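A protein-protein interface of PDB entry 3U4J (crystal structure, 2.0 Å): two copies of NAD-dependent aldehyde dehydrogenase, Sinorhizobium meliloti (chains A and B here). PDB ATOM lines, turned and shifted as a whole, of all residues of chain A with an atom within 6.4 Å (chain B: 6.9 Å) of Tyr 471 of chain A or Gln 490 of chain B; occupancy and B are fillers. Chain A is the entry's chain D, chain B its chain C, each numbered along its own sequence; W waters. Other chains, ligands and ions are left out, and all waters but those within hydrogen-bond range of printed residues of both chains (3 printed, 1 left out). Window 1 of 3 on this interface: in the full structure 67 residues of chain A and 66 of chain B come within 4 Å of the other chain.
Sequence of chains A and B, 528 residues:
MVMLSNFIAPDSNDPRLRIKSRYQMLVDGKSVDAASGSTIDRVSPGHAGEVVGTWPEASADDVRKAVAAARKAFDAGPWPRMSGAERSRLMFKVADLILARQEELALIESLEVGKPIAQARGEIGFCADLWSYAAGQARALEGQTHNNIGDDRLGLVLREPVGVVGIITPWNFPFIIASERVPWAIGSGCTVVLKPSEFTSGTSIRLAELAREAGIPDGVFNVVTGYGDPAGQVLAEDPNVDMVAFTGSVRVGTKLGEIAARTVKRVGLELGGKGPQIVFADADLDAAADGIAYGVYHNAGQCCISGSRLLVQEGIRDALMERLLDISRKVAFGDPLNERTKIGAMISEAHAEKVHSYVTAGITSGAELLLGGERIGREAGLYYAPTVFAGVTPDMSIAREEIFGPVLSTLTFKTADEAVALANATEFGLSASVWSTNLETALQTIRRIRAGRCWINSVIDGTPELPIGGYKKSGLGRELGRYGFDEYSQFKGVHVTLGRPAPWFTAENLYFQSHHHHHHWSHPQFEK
The backbone carbonyl oxygen (O) of Phe 491 of chain B sits at hydrogen-bond distance from the guanidinium group (NE) of Arg 478 of chain A (2.9 Å). The backbone NH (N) of Gly 493 of chain B sits at hydrogen-bond distance from the backbone carbonyl oxygen (O) of Gly 452 of chain A, at 2.8 Å. OH of Tyr 471 of chain A lies within hydrogen-bond range of OE1 of Glu 160 of chain B, 2.5 Å away. NH2 of Arg 478 of chain A lies close to NE2 of Gln 490 of chain B (2.9 Å). The side-chain amino group (NZ) of Lys 492 of chain B is in hydrogen-bond range of the backbone carbonyl oxygen (O) of Ile 449 of chain A.
O of Gly 429 of chain A is in hydrogen-bond range of N of Gly 452 of chain A (3.2 Å). NZ of Lys 473 of chain A lies within salt-bridge range of OE1 of Glu 427 of chain A (2.8 Å). The backbone carbonyl oxygen (O) of Leu 430 of chain A sits at hydrogen-bond distance from the backbone NH (N) of Arg 453 of chain A, at 2.8 Å. The backbone carbonyl oxygen (O) of Phe 428 of chain A sits close to the side-chain amino group (NZ) of Lys 472 of chain A, 3.5 Å away. O of Gly 470 of chain A sits at hydrogen-bond distance from NH1 of Arg 478 of chain A (3.1 Å). N of Leu 158 of chain B lies within hydrogen-bond range of O of Lys 492 of chain B (2.8 Å).
Ala 451 of chain A touches Lys 492 of chain B. Gly 452 of chain A touches Phe 491 of chain B (O to O, 3.9 Å). CA of Lys 492 of chain B touches O of Gly 452 of chain A, at 3.5 Å. O of Gly 493 of chain B touches C of Arg 453 of chain A, at 3.6 Å. Gln 490 of chain B touches Gly 470 of chain A. Gln 490 of chain B touches Tyr 471 of chain A. CB of Lys 492 of chain B touches OH of Tyr 471 of chain A, at 3.7 Å. O of Val 264 of chain B touches O of Lys 472 of chain A (3.9 Å). Val 264 of chain B touches Lys 473 of chain A (CB to CA, 3.97 Å).
Of the printed residues of chain B, Ile 449 of chain A touches Lys 492. Printed residues of chain B within 4 Å of Gly 470 of chain A: Gln 490. Tyr 471 of chain A touches three residues of chain B. Of the printed residues of chain B, Lys 472 of chain A touches Val 264. Asp 242 of chain B touches none of the printed residues of chain A. Of chain A, only Gly 470 (3.7 Å), Tyr 471 (3.4 Å) and Arg 478 (2.9 Å) come within 4 Å of Gln 490 of chain B. The nearest printed residue of chain B that does not touch Gly 470 of chain A is Arg 266 of chain B (6.0 Å).
Hydrophobic or aromatic side chains of chain B that line the printed part of chain A: Val 264. Among the printed residues, 14 pairs touch across the chains. Among the printed residues, no Asp or Glu carboxylate lies within 4 Å of a Lys or Arg side-chain nitrogen of the other chain.
No position is printed for both chains. Of the 14 pairs that touch across the chains among the printed residues, none has its exchanged pair printed and touching as well.
Water W1 lies within hydrogen-bond range of the side-chain carboxylate of Glu 160 of chain B, the side-chain amino group of Lys 492 of chain B and the backbone carbonyl oxygen of Ile 449 of chain A. Water W3 lies within hydrogen-bond range of O of Gly 452 of chain A (3.0 Å), NE of Arg 478 of chain A (3.1 Å) and O of Phe 491 of chain B (3.4 Å). Water W2 bridges OD1 of Asp 242 of chain B (3.1 Å) and NH1 of Arg 450 of chain A (3.5 Å).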
ATOM      1  N   GLU A 427      -9.095  16.014 -27.442  1.00  0.00           N
ATOM      2  CA  GLU A 427      -9.675  17.314 -27.064  1.00  0.00           C
ATOM      3  C   GLU A 427      -9.076  17.800 -25.742  1.00  0.00           C
ATOM      4  O   GLU A 427      -9.344  18.930 -25.315  1.00  0.00           O
ATOM      5  CB  GLU A 427     -11.211  17.259 -26.973  1.00  0.00           C
ATOM      6  CG  GLU A 427     -11.894  17.017 -28.328  1.00  0.00           C
ATOM      7  CD  GLU A 427     -13.421  16.936 -28.273  1.00  0.00           C
ATOM      8  OE1 GLU A 427     -14.054  17.421 -27.304  1.00  0.00           O
ATOM      9  OE2 GLU A 427     -13.995  16.394 -29.247  1.00  0.00           O
ATOM     10  N   PHE A 428      -8.286  16.954 -25.083  1.00  0.00           N
ATOM     11  CA  PHE A 428      -7.695  17.338 -23.782  1.00  0.00           C
ATOM     12  C   PHE A 428      -6.299  17.934 -23.972  1.00  0.00           C
ATOM     13  O   PHE A 428      -5.750  17.901 -25.075  1.00  0.00           O
ATOM     14  CB  PHE A 428      -7.602  16.146 -22.819  1.00  0.00           C
ATOM     15  CG  PHE A 428      -8.928  15.448 -22.554  1.00  0.00           C
ATOM     16  CD1 PHE A 428      -9.889  16.027 -21.742  1.00  0.00           C
ATOM     17  CD2 PHE A 428      -9.193  14.201 -23.115  1.00  0.00           C
ATOM     18  CE1 PHE A 428     -11.106  15.378 -21.480  1.00  0.00           C
ATOM     19  CE2 PHE A 428     -10.401  13.542 -22.876  1.00  0.00           C
ATOM     20  CZ  PHE A 428     -11.363  14.134 -22.051  1.00  0.00           C
ATOM     21  N   GLY A 429      -5.732  18.482 -22.896  1.00  0.00           N
ATOM     22  CA  GLY A 429      -4.399  19.047 -22.968  1.00  0.00           C
ATOM     23  C   GLY A 429      -3.866  19.373 -21.591  1.00  0.00           C
ATOM     24  O   GLY A 429      -3.325  20.452 -21.379  1.00  0.00           O
ATOM     25  N   LEU A 430      -4.027  18.445 -20.646  1.00  0.00           N
ATOM     26  CA  LEU A 430      -3.605  18.725 -19.278  1.00  0.00           C
ATOM     27  C   LEU A 430      -2.129  18.382 -19.062  1.00  0.00           C
ATOM     28  O   LEU A 430      -1.365  19.233 -18.631  1.00  0.00           O
ATOM     29  CB  LEU A 430      -4.501  18.024 -18.231  1.00  0.00           C
ATOM     30  CG  LEU A 430      -4.191  18.383 -16.753  1.00  0.00           C
ATOM     31  CD1 LEU A 430      -4.305  19.908 -16.455  1.00  0.00           C
ATOM     32  CD2 LEU A 430      -5.101  17.583 -15.796  1.00  0.00           C
ATOM     33  N   ILE A 449       3.935  19.375 -28.025  1.00  0.00           N
ATOM     34  CA  ILE A 449       2.720  18.838 -27.417  1.00  0.00           C
ATOM     35  C   ILE A 449       1.921  19.952 -26.717  1.00  0.00           C
ATOM     36  O   ILE A 449       2.456  20.705 -25.894  1.00  0.00           O
ATOM     37  CB  ILE A 449       3.055  17.697 -26.437  1.00  0.00           C
ATOM     38  CG1 ILE A 449       3.558  16.483 -27.222  1.00  0.00           C
ATOM     39  CG2 ILE A 449       1.845  17.299 -25.577  1.00  0.00           C
ATOM     40  CD1 ILE A 449       4.310  15.511 -26.382  1.00  0.00           C
ATOM     41  N   ARG A 450       0.640  20.036 -27.050  1.00  0.00           N
ATOM     42  CA  ARG A 450      -0.231  21.062 -26.521  1.00  0.00           C
ATOM     43  C   ARG A 450      -0.810  20.630 -25.168  1.00  0.00           C
ATOM     44  O   ARG A 450      -1.942  20.161 -25.071  1.00  0.00           O
ATOM     45  CB  ARG A 450      -1.311  21.357 -27.563  1.00  0.00           C
ATOM     46  CG  ARG A 450      -0.706  21.922 -28.859  1.00  0.00           C
ATOM     47  CD  ARG A 450      -1.773  22.150 -29.927  1.00  0.00           C
ATOM     48  NE  ARG A 450      -1.177  22.621 -31.186  1.00  0.00           N
ATOM     49  CZ  ARG A 450      -1.854  22.883 -32.306  1.00  0.00           C
ATOM     50  NH1 ARG A 450      -3.168  22.714 -32.352  1.00  0.00           N
ATOM     51  NH2 ARG A 450      -1.206  23.313 -33.382  1.00  0.00           N
ATOM     52  N   ALA A 451       0.003  20.747 -24.126  1.00  0.00           N
ATOM     53  CA  ALA A 451      -0.387  20.302 -22.803  1.00  0.00           C
ATOM     54  C   ALA A 451       0.278  21.244 -21.810  1.00  0.00           C
ATOM     55  O   ALA A 451       1.415  21.657 -22.047  1.00  0.00           O
ATOM     56  CB  ALA A 451       0.069  18.846 -22.577  1.00  0.00           C
ATOM     57  N   GLY A 452      -0.431  21.600 -20.735  1.00  0.00           N
ATOM     58  CA  GLY A 452       0.073  22.609 -19.798  1.00  0.00           C
ATOM     59  C   GLY A 452       1.036  22.112 -18.733  1.00  0.00           C
ATOM     60  O   GLY A 452       1.804  22.911 -18.155  1.00  0.00           O
ATOM     61  N   ARG A 453       0.974  20.809 -18.429  1.00  0.00           N
ATOM     62  CA  ARG A 453       1.754  20.226 -17.345  1.00  0.00           C
ATOM     63  C   ARG A 453       2.597  19.122 -17.947  1.00  0.00           C
ATOM     64  O   ARG A 453       2.108  18.019 -18.221  1.00  0.00           O
ATOM     65  CB  ARG A 453       0.842  19.652 -16.247  1.00  0.00           C
ATOM     66  CG  ARG A 453       0.006  20.682 -15.494  1.00  0.00           C
ATOM     67  CD  ARG A 453      -0.885  20.008 -14.453  1.00  0.00           C
ATOM     68  NE  ARG A 453      -0.181  19.615 -13.211  1.00  0.00           N
ATOM     69  CZ  ARG A 453      -0.818  19.226 -12.099  1.00  0.00           C
ATOM     70  NH1 ARG A 453      -2.144  19.190 -12.076  1.00  0.00           N
ATOM     71  NH2 ARG A 453      -0.145  18.893 -11.000  1.00  0.00           N
ATOM     72  N   GLY A 469      -1.793  23.896 -15.045  1.00  0.00           N
ATOM     73  CA  GLY A 469      -3.100  24.142 -15.687  1.00  0.00           C
ATOM     74  C   GLY A 469      -3.131  23.469 -17.055  1.00  0.00           C
ATOM     75  O   GLY A 469      -2.125  22.918 -17.495  1.00  0.00           O
ATOM     76  N   GLY A 470      -4.279  23.517 -17.735  1.00  0.00           N
ATOM     77  CA  GLY A 470      -4.427  22.802 -19.003  1.00  0.00           C
ATOM     78  C   GLY A 470      -4.470  23.669 -20.250  1.00  0.00           C
ATOM     79  O   GLY A 470      -4.715  24.877 -20.166  1.00  0.00           O
ATOM     80  N   TYR A 471      -4.216  23.052 -21.400  1.00  0.00           N
ATOM     81  CA  TYR A 471      -4.640  23.611 -22.711  1.00  0.00           C
ATOM     82  C   TYR A 471      -5.990  23.007 -23.086  1.00  0.00           C
ATOM     83  O   TYR A 471      -6.440  22.048 -22.459  1.00  0.00           O
ATOM     84  CB  TYR A 471      -3.666  23.212 -23.818  1.00  0.00           C
ATOM     85  CG  TYR A 471      -2.279  23.886 -23.845  1.00  0.00           C
ATOM     86  CD1 TYR A 471      -1.673  24.197 -25.069  1.00  0.00           C
ATOM     87  CD2 TYR A 471      -1.584  24.186 -22.672  1.00  0.00           C
ATOM     88  CE1 TYR A 471      -0.394  24.779 -25.127  1.00  0.00           C
ATOM     89  CE2 TYR A 471      -0.281  24.776 -22.718  1.00  0.00           C
ATOM     90  CZ  TYR A 471       0.283  25.060 -23.938  1.00  0.00           C
ATOM     91  OH  TYR A 471       1.523  25.646 -23.988  1.00  0.00           O
ATOM     92  N   LYS A 472      -6.608  23.561 -24.130  1.00  0.00           N
ATOM     93  CA  LYS A 472      -7.764  22.959 -24.790  1.00  0.00           C
ATOM     94  C   LYS A 472      -8.893  22.752 -23.763  1.00  0.00           C
ATOM     95  O   LYS A 472      -9.191  23.658 -22.990  1.00  0.00           O
ATOM     96  CB  LYS A 472      -7.338  21.651 -25.496  1.00  0.00           C
ATOM     97  CG  LYS A 472      -6.421  21.865 -26.722  1.00  0.00           C
ATOM     98  CD  LYS A 472      -6.475  20.667 -27.675  1.00  0.00           C
ATOM     99  CE  LYS A 472      -5.188  19.925 -27.630  1.00  0.00           C
ATOM    100  NZ  LYS A 472      -5.201  18.661 -28.426  1.00  0.00           N
ATOM    101  N   LYS A 473      -9.513  21.575 -23.725  1.00  0.00           N
ATOM    102  CA  LYS A 473     -10.668  21.371 -22.808  1.00  0.00           C
ATOM    103  C   LYS A 473     -10.279  20.943 -21.369  1.00  0.00           C
ATOM    104  O   LYS A 473     -11.148  20.661 -20.538  1.00  0.00           O
ATOM    105  CB  LYS A 473     -11.690  20.392 -23.415  1.00  0.00           C
ATOM    106  CG  LYS A 473     -12.349  20.903 -24.706  1.00  0.00           C
ATOM    107  CD  LYS A 473     -13.590  20.086 -25.062  1.00  0.00           C
ATOM    108  CE  LYS A 473     -14.258  20.638 -26.325  1.00  0.00           C
ATOM    109  NZ  LYS A 473     -15.397  19.762 -26.741  1.00  0.00           N
ATOM    110  N   SER A 474      -8.982  20.912 -21.067  1.00  0.00           N
ATOM    111  CA  SER A 474      -8.546  20.504 -19.734  1.00  0.00           C
ATOM    112  C   SER A 474      -8.502  21.624 -18.684  1.00  0.00           C
ATOM    113  O   SER A 474      -8.180  21.369 -17.519  1.00  0.00           O
ATOM    114  CB  SER A 474      -7.191  19.802 -19.788  1.00  0.00           C
ATOM    115  OG  SER A 474      -7.288  18.617 -20.554  1.00  0.00           O
ATOM    116  N   GLY A 475      -8.815  22.851 -19.076  1.00  0.00           N
ATOM    117  CA  GLY A 475      -8.888  23.918 -18.085  1.00  0.00           C
ATOM    118  C   GLY A 475      -8.798  25.341 -18.570  1.00  0.00           C
ATOM    119  O   GLY A 475      -8.558  25.594 -19.758  1.00  0.00           O
ATOM    120  N   GLY A 477      -7.003  29.034 -16.981  1.00  0.00           N
ATOM    121  CA  GLY A 477      -6.206  29.657 -15.937  1.00  0.00           C
ATOM    122  C   GLY A 477      -5.007  28.808 -15.539  1.00  0.00           C
ATOM    123  O   GLY A 477      -4.793  27.727 -16.081  1.00  0.00           O
ATOM    124  N   ARG A 478      -4.243  29.307 -14.569  1.00  0.00           N
ATOM    125  CA  ARG A 478      -3.022  28.667 -14.084  1.00  0.00           C
ATOM    126  C   ARG A 478      -2.940  28.852 -12.579  1.00  0.00           C
ATOM    127  O   ARG A 478      -3.136  29.958 -12.070  1.00  0.00           O
ATOM    128  CB  ARG A 478      -1.748  29.262 -14.726  1.00  0.00           C
ATOM    129  CG  ARG A 478      -1.473  28.856 -16.176  1.00  0.00           C
ATOM    130  CD  ARG A 478      -1.250  27.349 -16.304  1.00  0.00           C
ATOM    131  NE  ARG A 478      -1.003  26.876 -17.666  1.00  0.00           N
ATOM    132  CZ  ARG A 478      -1.952  26.643 -18.575  1.00  0.00           C
ATOM    133  NH1 ARG A 478      -3.249  26.860 -18.290  1.00  0.00           N
ATOM    134  NH2 ARG A 478      -1.603  26.187 -19.779  1.00  0.00           N
ATOM    135  N   LEU B 158       7.395  27.492 -20.322  1.00  0.00           N
ATOM    136  CA  LEU B 158       7.500  27.963 -21.700  1.00  0.00           C
ATOM    137  C   LEU B 158       6.236  28.725 -22.104  1.00  0.00           C
ATOM    138  O   LEU B 158       5.127  28.259 -21.873  1.00  0.00           O
ATOM    139  CB  LEU B 158       7.740  26.787 -22.671  1.00  0.00           C
ATOM    140  CG  LEU B 158       8.986  25.913 -22.457  1.00  0.00           C
ATOM    141  CD1 LEU B 158       8.974  24.636 -23.321  1.00  0.00           C
ATOM    142  CD2 LEU B 158      10.247  26.728 -22.717  1.00  0.00           C
ATOM    143  N   ARG B 159       6.419  29.896 -22.700  1.00  0.00           N
ATOM    144  CA  ARG B 159       5.315  30.694 -23.192  1.00  0.00           C
ATOM    145  C   ARG B 159       5.023  30.266 -24.635  1.00  0.00           C
ATOM    146  O   ARG B 159       5.935  30.192 -25.454  1.00  0.00           O
ATOM    147  CB  ARG B 159       5.660  32.207 -23.138  1.00  0.00           C
ATOM    148  CG  ARG B 159       4.632  33.079 -23.885  1.00  0.00           C
ATOM    149  CD  ARG B 159       5.045  34.563 -23.942  1.00  0.00           C
ATOM    150  NE  ARG B 159       5.259  35.157 -22.618  1.00  0.00           N
ATOM    151  CZ  ARG B 159       4.358  35.889 -21.963  1.00  0.00           C
ATOM    152  NH1 ARG B 159       3.149  36.103 -22.490  1.00  0.00           N
ATOM    153  NH2 ARG B 159       4.655  36.391 -20.764  1.00  0.00           N
ATOM    154  N   GLU B 160       3.751  29.983 -24.933  1.00  0.00           N
ATOM    155  CA  GLU B 160       3.338  29.601 -26.290  1.00  0.00           C
ATOM    156  C   GLU B 160       2.067  30.351 -26.664  1.00  0.00           C
ATOM    157  O   GLU B 160       1.372  30.848 -25.793  1.00  0.00           O
ATOM    158  CB  GLU B 160       3.079  28.083 -26.341  1.00  0.00           C
ATOM    159  CG  GLU B 160       4.303  27.227 -25.920  1.00  0.00           C
ATOM    160  CD  GLU B 160       4.020  25.738 -26.005  1.00  0.00           C
ATOM    161  OE1 GLU B 160       2.829  25.365 -26.143  1.00  0.00           O
ATOM    162  OE2 GLU B 160       4.979  24.943 -25.942  1.00  0.00           O
ATOM    163  N   PRO B 161       1.729  30.408 -27.958  1.00  0.00           N
ATOM    164  CA  PRO B 161       0.477  31.062 -28.343  1.00  0.00           C
ATOM    165  C   PRO B 161      -0.765  30.281 -27.916  1.00  0.00           C
ATOM    166  O   PRO B 161      -0.741  29.065 -27.848  1.00  0.00           O
ATOM    167  CB  PRO B 161       0.547  31.116 -29.872  1.00  0.00           C
ATOM    168  CG  PRO B 161       1.968  30.681 -30.225  1.00  0.00           C
ATOM    169  CD  PRO B 161       2.456  29.851 -29.118  1.00  0.00           C
ATOM    170  N   VAL B 162      -1.833  31.015 -27.627  1.00  0.00           N
ATOM    171  CA  VAL B 162      -3.178  30.475 -27.433  1.00  0.00           C
ATOM    172  C   VAL B 162      -3.669  29.714 -28.666  1.00  0.00           C
ATOM    173  O   VAL B 162      -4.242  28.629 -28.541  1.00  0.00           O
ATOM    174  CB  VAL B 162      -4.150  31.643 -26.996  1.00  0.00           C
ATOM    175  CG1 VAL B 162      -5.589  31.461 -27.499  1.00  0.00           C
ATOM    176  CG2 VAL B 162      -4.150  31.751 -25.497  1.00  0.00           C
ATOM    177  N   GLY B 163      -3.446  30.264 -29.855  1.00  0.00           N
ATOM    178  CA  GLY B 163      -3.824  29.580 -31.092  1.00  0.00           C
ATOM    179  C   GLY B 163      -4.695  30.465 -31.957  1.00  0.00           C
ATOM    180  O   GLY B 163      -4.265  31.544 -32.359  1.00  0.00           O
ATOM    181  N   ASP B 242      -9.811  28.887 -30.482  1.00  0.00           N
ATOM    182  CA  ASP B 242      -9.302  28.607 -29.151  1.00  0.00           C
ATOM    183  C   ASP B 242      -9.707  29.645 -28.128  1.00  0.00           C
ATOM    184  O   ASP B 242      -9.719  29.371 -26.945  1.00  0.00           O
ATOM    185  CB  ASP B 242      -7.792  28.494 -29.198  1.00  0.00           C
ATOM    186  CG  ASP B 242      -7.349  27.381 -30.102  1.00  0.00           C
ATOM    187  OD1 ASP B 242      -6.596  27.645 -31.050  1.00  0.00           O
ATOM    188  OD2 ASP B 242      -7.777  26.230 -29.866  1.00  0.00           O
ATOM    189  N   VAL B 264     -15.281  25.088 -23.166  1.00  0.00           N
ATOM    190  CA  VAL B 264     -14.119  25.488 -22.361  1.00  0.00           C
ATOM    191  C   VAL B 264     -13.255  26.454 -23.193  1.00  0.00           C
ATOM    192  O   VAL B 264     -12.030  26.387 -23.182  1.00  0.00           O
ATOM    193  CB  VAL B 264     -13.271  24.241 -21.925  1.00  0.00           C
ATOM    194  CG1 VAL B 264     -12.377  24.573 -20.714  1.00  0.00           C
ATOM    195  CG2 VAL B 264     -14.167  23.044 -21.643  1.00  0.00           C
ATOM    196  N   ARG B 266     -11.360  29.810 -24.110  1.00  0.00           N
ATOM    197  CA  ARG B 266     -10.914  31.009 -23.396  1.00  0.00           C
ATOM    198  C   ARG B 266     -11.711  32.231 -23.865  1.00  0.00           C
ATOM    199  O   ARG B 266     -12.059  32.329 -25.029  1.00  0.00           O
ATOM    200  CB  ARG B 266      -9.424  31.267 -23.541  1.00  0.00           C
ATOM    201  CG  ARG B 266      -8.996  32.335 -22.541  1.00  0.00           C
ATOM    202  CD  ARG B 266      -7.525  32.699 -22.565  1.00  0.00           C
ATOM    203  NE  ARG B 266      -6.657  31.587 -22.229  1.00  0.00           N
ATOM    204  CZ  ARG B 266      -5.329  31.690 -22.174  1.00  0.00           C
ATOM    205  NH1 ARG B 266      -4.727  32.858 -22.408  1.00  0.00           N
ATOM    206  NH2 ARG B 266      -4.604  30.625 -21.880  1.00  0.00           N
ATOM    207  N   PHE B 485      -0.217  40.312 -23.689  1.00  0.00           N
ATOM    208  CA  PHE B 485       0.472  39.140 -24.245  1.00  0.00           C
ATOM    209  C   PHE B 485       0.180  37.861 -23.461  1.00  0.00           C
ATOM    210  O   PHE B 485       0.107  36.759 -24.046  1.00  0.00           O
ATOM    211  CB  PHE B 485       1.992  39.358 -24.347  1.00  0.00           C
ATOM    212  CG  PHE B 485       2.370  40.441 -25.293  1.00  0.00           C
ATOM    213  CD1 PHE B 485       2.263  40.264 -26.661  1.00  0.00           C
ATOM    214  CD2 PHE B 485       2.776  41.686 -24.803  1.00  0.00           C
ATOM    215  CE1 PHE B 485       2.616  41.305 -27.553  1.00  0.00           C
ATOM    216  CE2 PHE B 485       3.139  42.710 -25.669  1.00  0.00           C
ATOM    217  CZ  PHE B 485       3.033  42.523 -27.051  1.00  0.00           C
ATOM    218  N   ASP B 486       0.010  38.010 -22.148  1.00  0.00           N
ATOM    219  CA  ASP B 486      -0.410  36.900 -21.302  1.00  0.00           C
ATOM    220  C   ASP B 486      -1.833  36.429 -21.649  1.00  0.00           C
ATOM    221  O   ASP B 486      -2.111  35.241 -21.590  1.00  0.00           O
ATOM    222  CB  ASP B 486      -0.291  37.249 -19.820  1.00  0.00           C
ATOM    223  CG  ASP B 486       1.153  37.507 -19.410  1.00  0.00           C
ATOM    224  OD1 ASP B 486       2.064  37.280 -20.238  1.00  0.00           O
ATOM    225  OD2 ASP B 486       1.374  38.013 -18.291  1.00  0.00           O
ATOM    226  N   GLU B 487      -2.713  37.354 -22.035  1.00  0.00           N
ATOM    227  CA  GLU B 487      -4.076  36.983 -22.487  1.00  0.00           C
ATOM    228  C   GLU B 487      -4.127  36.063 -23.709  1.00  0.00           C
ATOM    229  O   GLU B 487      -5.088  35.289 -23.872  1.00  0.00           O
ATOM    230  CB  GLU B 487      -4.907  38.224 -22.842  1.00  0.00           C
ATOM    231  CG  GLU B 487      -5.372  39.022 -21.690  1.00  0.00           C
ATOM    232  CD  GLU B 487      -6.296  38.276 -20.752  1.00  0.00           C
ATOM    233  OE1 GLU B 487      -7.295  37.673 -21.205  1.00  0.00           O
ATOM    234  OE2 GLU B 487      -6.018  38.329 -19.543  1.00  0.00           O
ATOM    235  N   TYR B 488      -3.124  36.179 -24.580  1.00  0.00           N
ATOM    236  CA  TYR B 488      -3.080  35.432 -25.826  1.00  0.00           C
ATOM    237  C   TYR B 488      -1.990  34.356 -25.794  1.00  0.00           C
ATOM    238  O   TYR B 488      -1.636  33.799 -26.832  1.00  0.00           O
ATOM    239  CB  TYR B 488      -2.912  36.389 -27.039  1.00  0.00           C
ATOM    240  CG  TYR B 488      -3.999  37.432 -27.043  1.00  0.00           C
ATOM    241  CD1 TYR B 488      -5.305  37.085 -27.362  1.00  0.00           C
ATOM    242  CD2 TYR B 488      -3.736  38.745 -26.648  1.00  0.00           C
ATOM    243  CE1 TYR B 488      -6.330  38.034 -27.312  1.00  0.00           C
ATOM    244  CE2 TYR B 488      -4.749  39.704 -26.605  1.00  0.00           C
ATOM    245  CZ  TYR B 488      -6.046  39.332 -26.932  1.00  0.00           C
ATOM    246  OH  TYR B 488      -7.080  40.232 -26.875  1.00  0.00           O
ATOM    247  N   SER B 489      -1.515  34.030 -24.598  1.00  0.00           N
ATOM    248  CA  SER B 489      -0.488  32.995 -24.423  1.00  0.00           C
ATOM    249  C   SER B 489      -1.033  31.840 -23.590  1.00  0.00           C
ATOM    250  O   SER B 489      -1.936  32.021 -22.762  1.00  0.00           O
ATOM    251  CB  SER B 489       0.762  33.559 -23.690  1.00  0.00           C
ATOM    252  OG  SER B 489       1.403  34.552 -24.467  1.00  0.00           O
ATOM    253  N   GLN B 490      -0.452  30.661 -23.793  1.00  0.00           N
ATOM    254  CA  GLN B 490      -0.574  29.548 -22.871  1.00  0.00           C
ATOM    255  C   GLN B 490       0.785  29.380 -22.226  1.00  0.00           C
ATOM    256  O   GLN B 490       1.822  29.601 -22.871  1.00  0.00           O
ATOM    257  CB  GLN B 490      -0.912  28.249 -23.625  1.00  0.00           C
ATOM    258  CG  GLN B 490      -2.348  28.152 -24.167  1.00  0.00           C
ATOM    259  CD  GLN B 490      -3.406  27.755 -23.115  1.00  0.00           C
ATOM    260  OE1 GLN B 490      -4.576  27.487 -23.461  1.00  0.00           O
ATOM    261  NE2 GLN B 490      -3.009  27.711 -21.851  1.00  0.00           N
ATOM    262  N   PHE B 491       0.794  28.948 -20.978  1.00  0.00           N
ATOM    263  CA  PHE B 491       2.047  28.667 -20.280  1.00  0.00           C
ATOM    264  C   PHE B 491       2.150  27.177 -19.980  1.00  0.00           C
ATOM    265  O   PHE B 491       1.223  26.582 -19.424  1.00  0.00           O
ATOM    266  CB  PHE B 491       2.135  29.501 -18.999  1.00  0.00           C
ATOM    267  CG  PHE B 491       2.170  30.966 -19.268  1.00  0.00           C
ATOM    268  CD1 PHE B 491       3.378  31.591 -19.557  1.00  0.00           C
ATOM    269  CD2 PHE B 491       1.002  31.714 -19.291  1.00  0.00           C
ATOM    270  CE1 PHE B 491       3.426  32.962 -19.834  1.00  0.00           C
ATOM    271  CE2 PHE B 491       1.037  33.103 -19.593  1.00  0.00           C
ATOM    272  CZ  PHE B 491       2.237  33.708 -19.868  1.00  0.00           C
ATOM    273  N   LYS B 492       3.268  26.593 -20.380  1.00  0.00           N
ATOM    274  CA  LYS B 492       3.536  25.181 -20.225  1.00  0.00           C
ATOM    275  C   LYS B 492       4.605  24.986 -19.156  1.00  0.00           C
ATOM    276  O   LYS B 492       5.735  25.470 -19.293  1.00  0.00           O
ATOM    277  CB  LYS B 492       4.050  24.632 -21.553  1.00  0.00           C
ATOM    278  CG  LYS B 492       4.484  23.156 -21.512  1.00  0.00           C
ATOM    279  CD  LYS B 492       5.062  22.736 -22.876  1.00  0.00           C
ATOM    280  CE  LYS B 492       3.890  22.569 -23.877  1.00  0.00           C
ATOM    281  NZ  LYS B 492       4.362  22.420 -25.269  1.00  0.00           N
ATOM    282  N   GLY B 493       4.244  24.289 -18.083  1.00  0.00           N
ATOM    283  CA  GLY B 493       5.199  24.011 -17.024  1.00  0.00           C
ATOM    284  C   GLY B 493       5.851  22.664 -17.285  1.00  0.00           C
ATOM    285  O   GLY B 493       5.161  21.655 -17.399  1.00  0.00           O
HETATM  286  O   HOH W   1       2.804  23.288 -28.189  1.00  0.00           O
HETATM  287  O   HOH W   2      -4.296  25.608 -30.742  1.00  0.00           O
HETATM  288  O   HOH W   3       1.232  25.209 -16.267  1.00  0.00           O
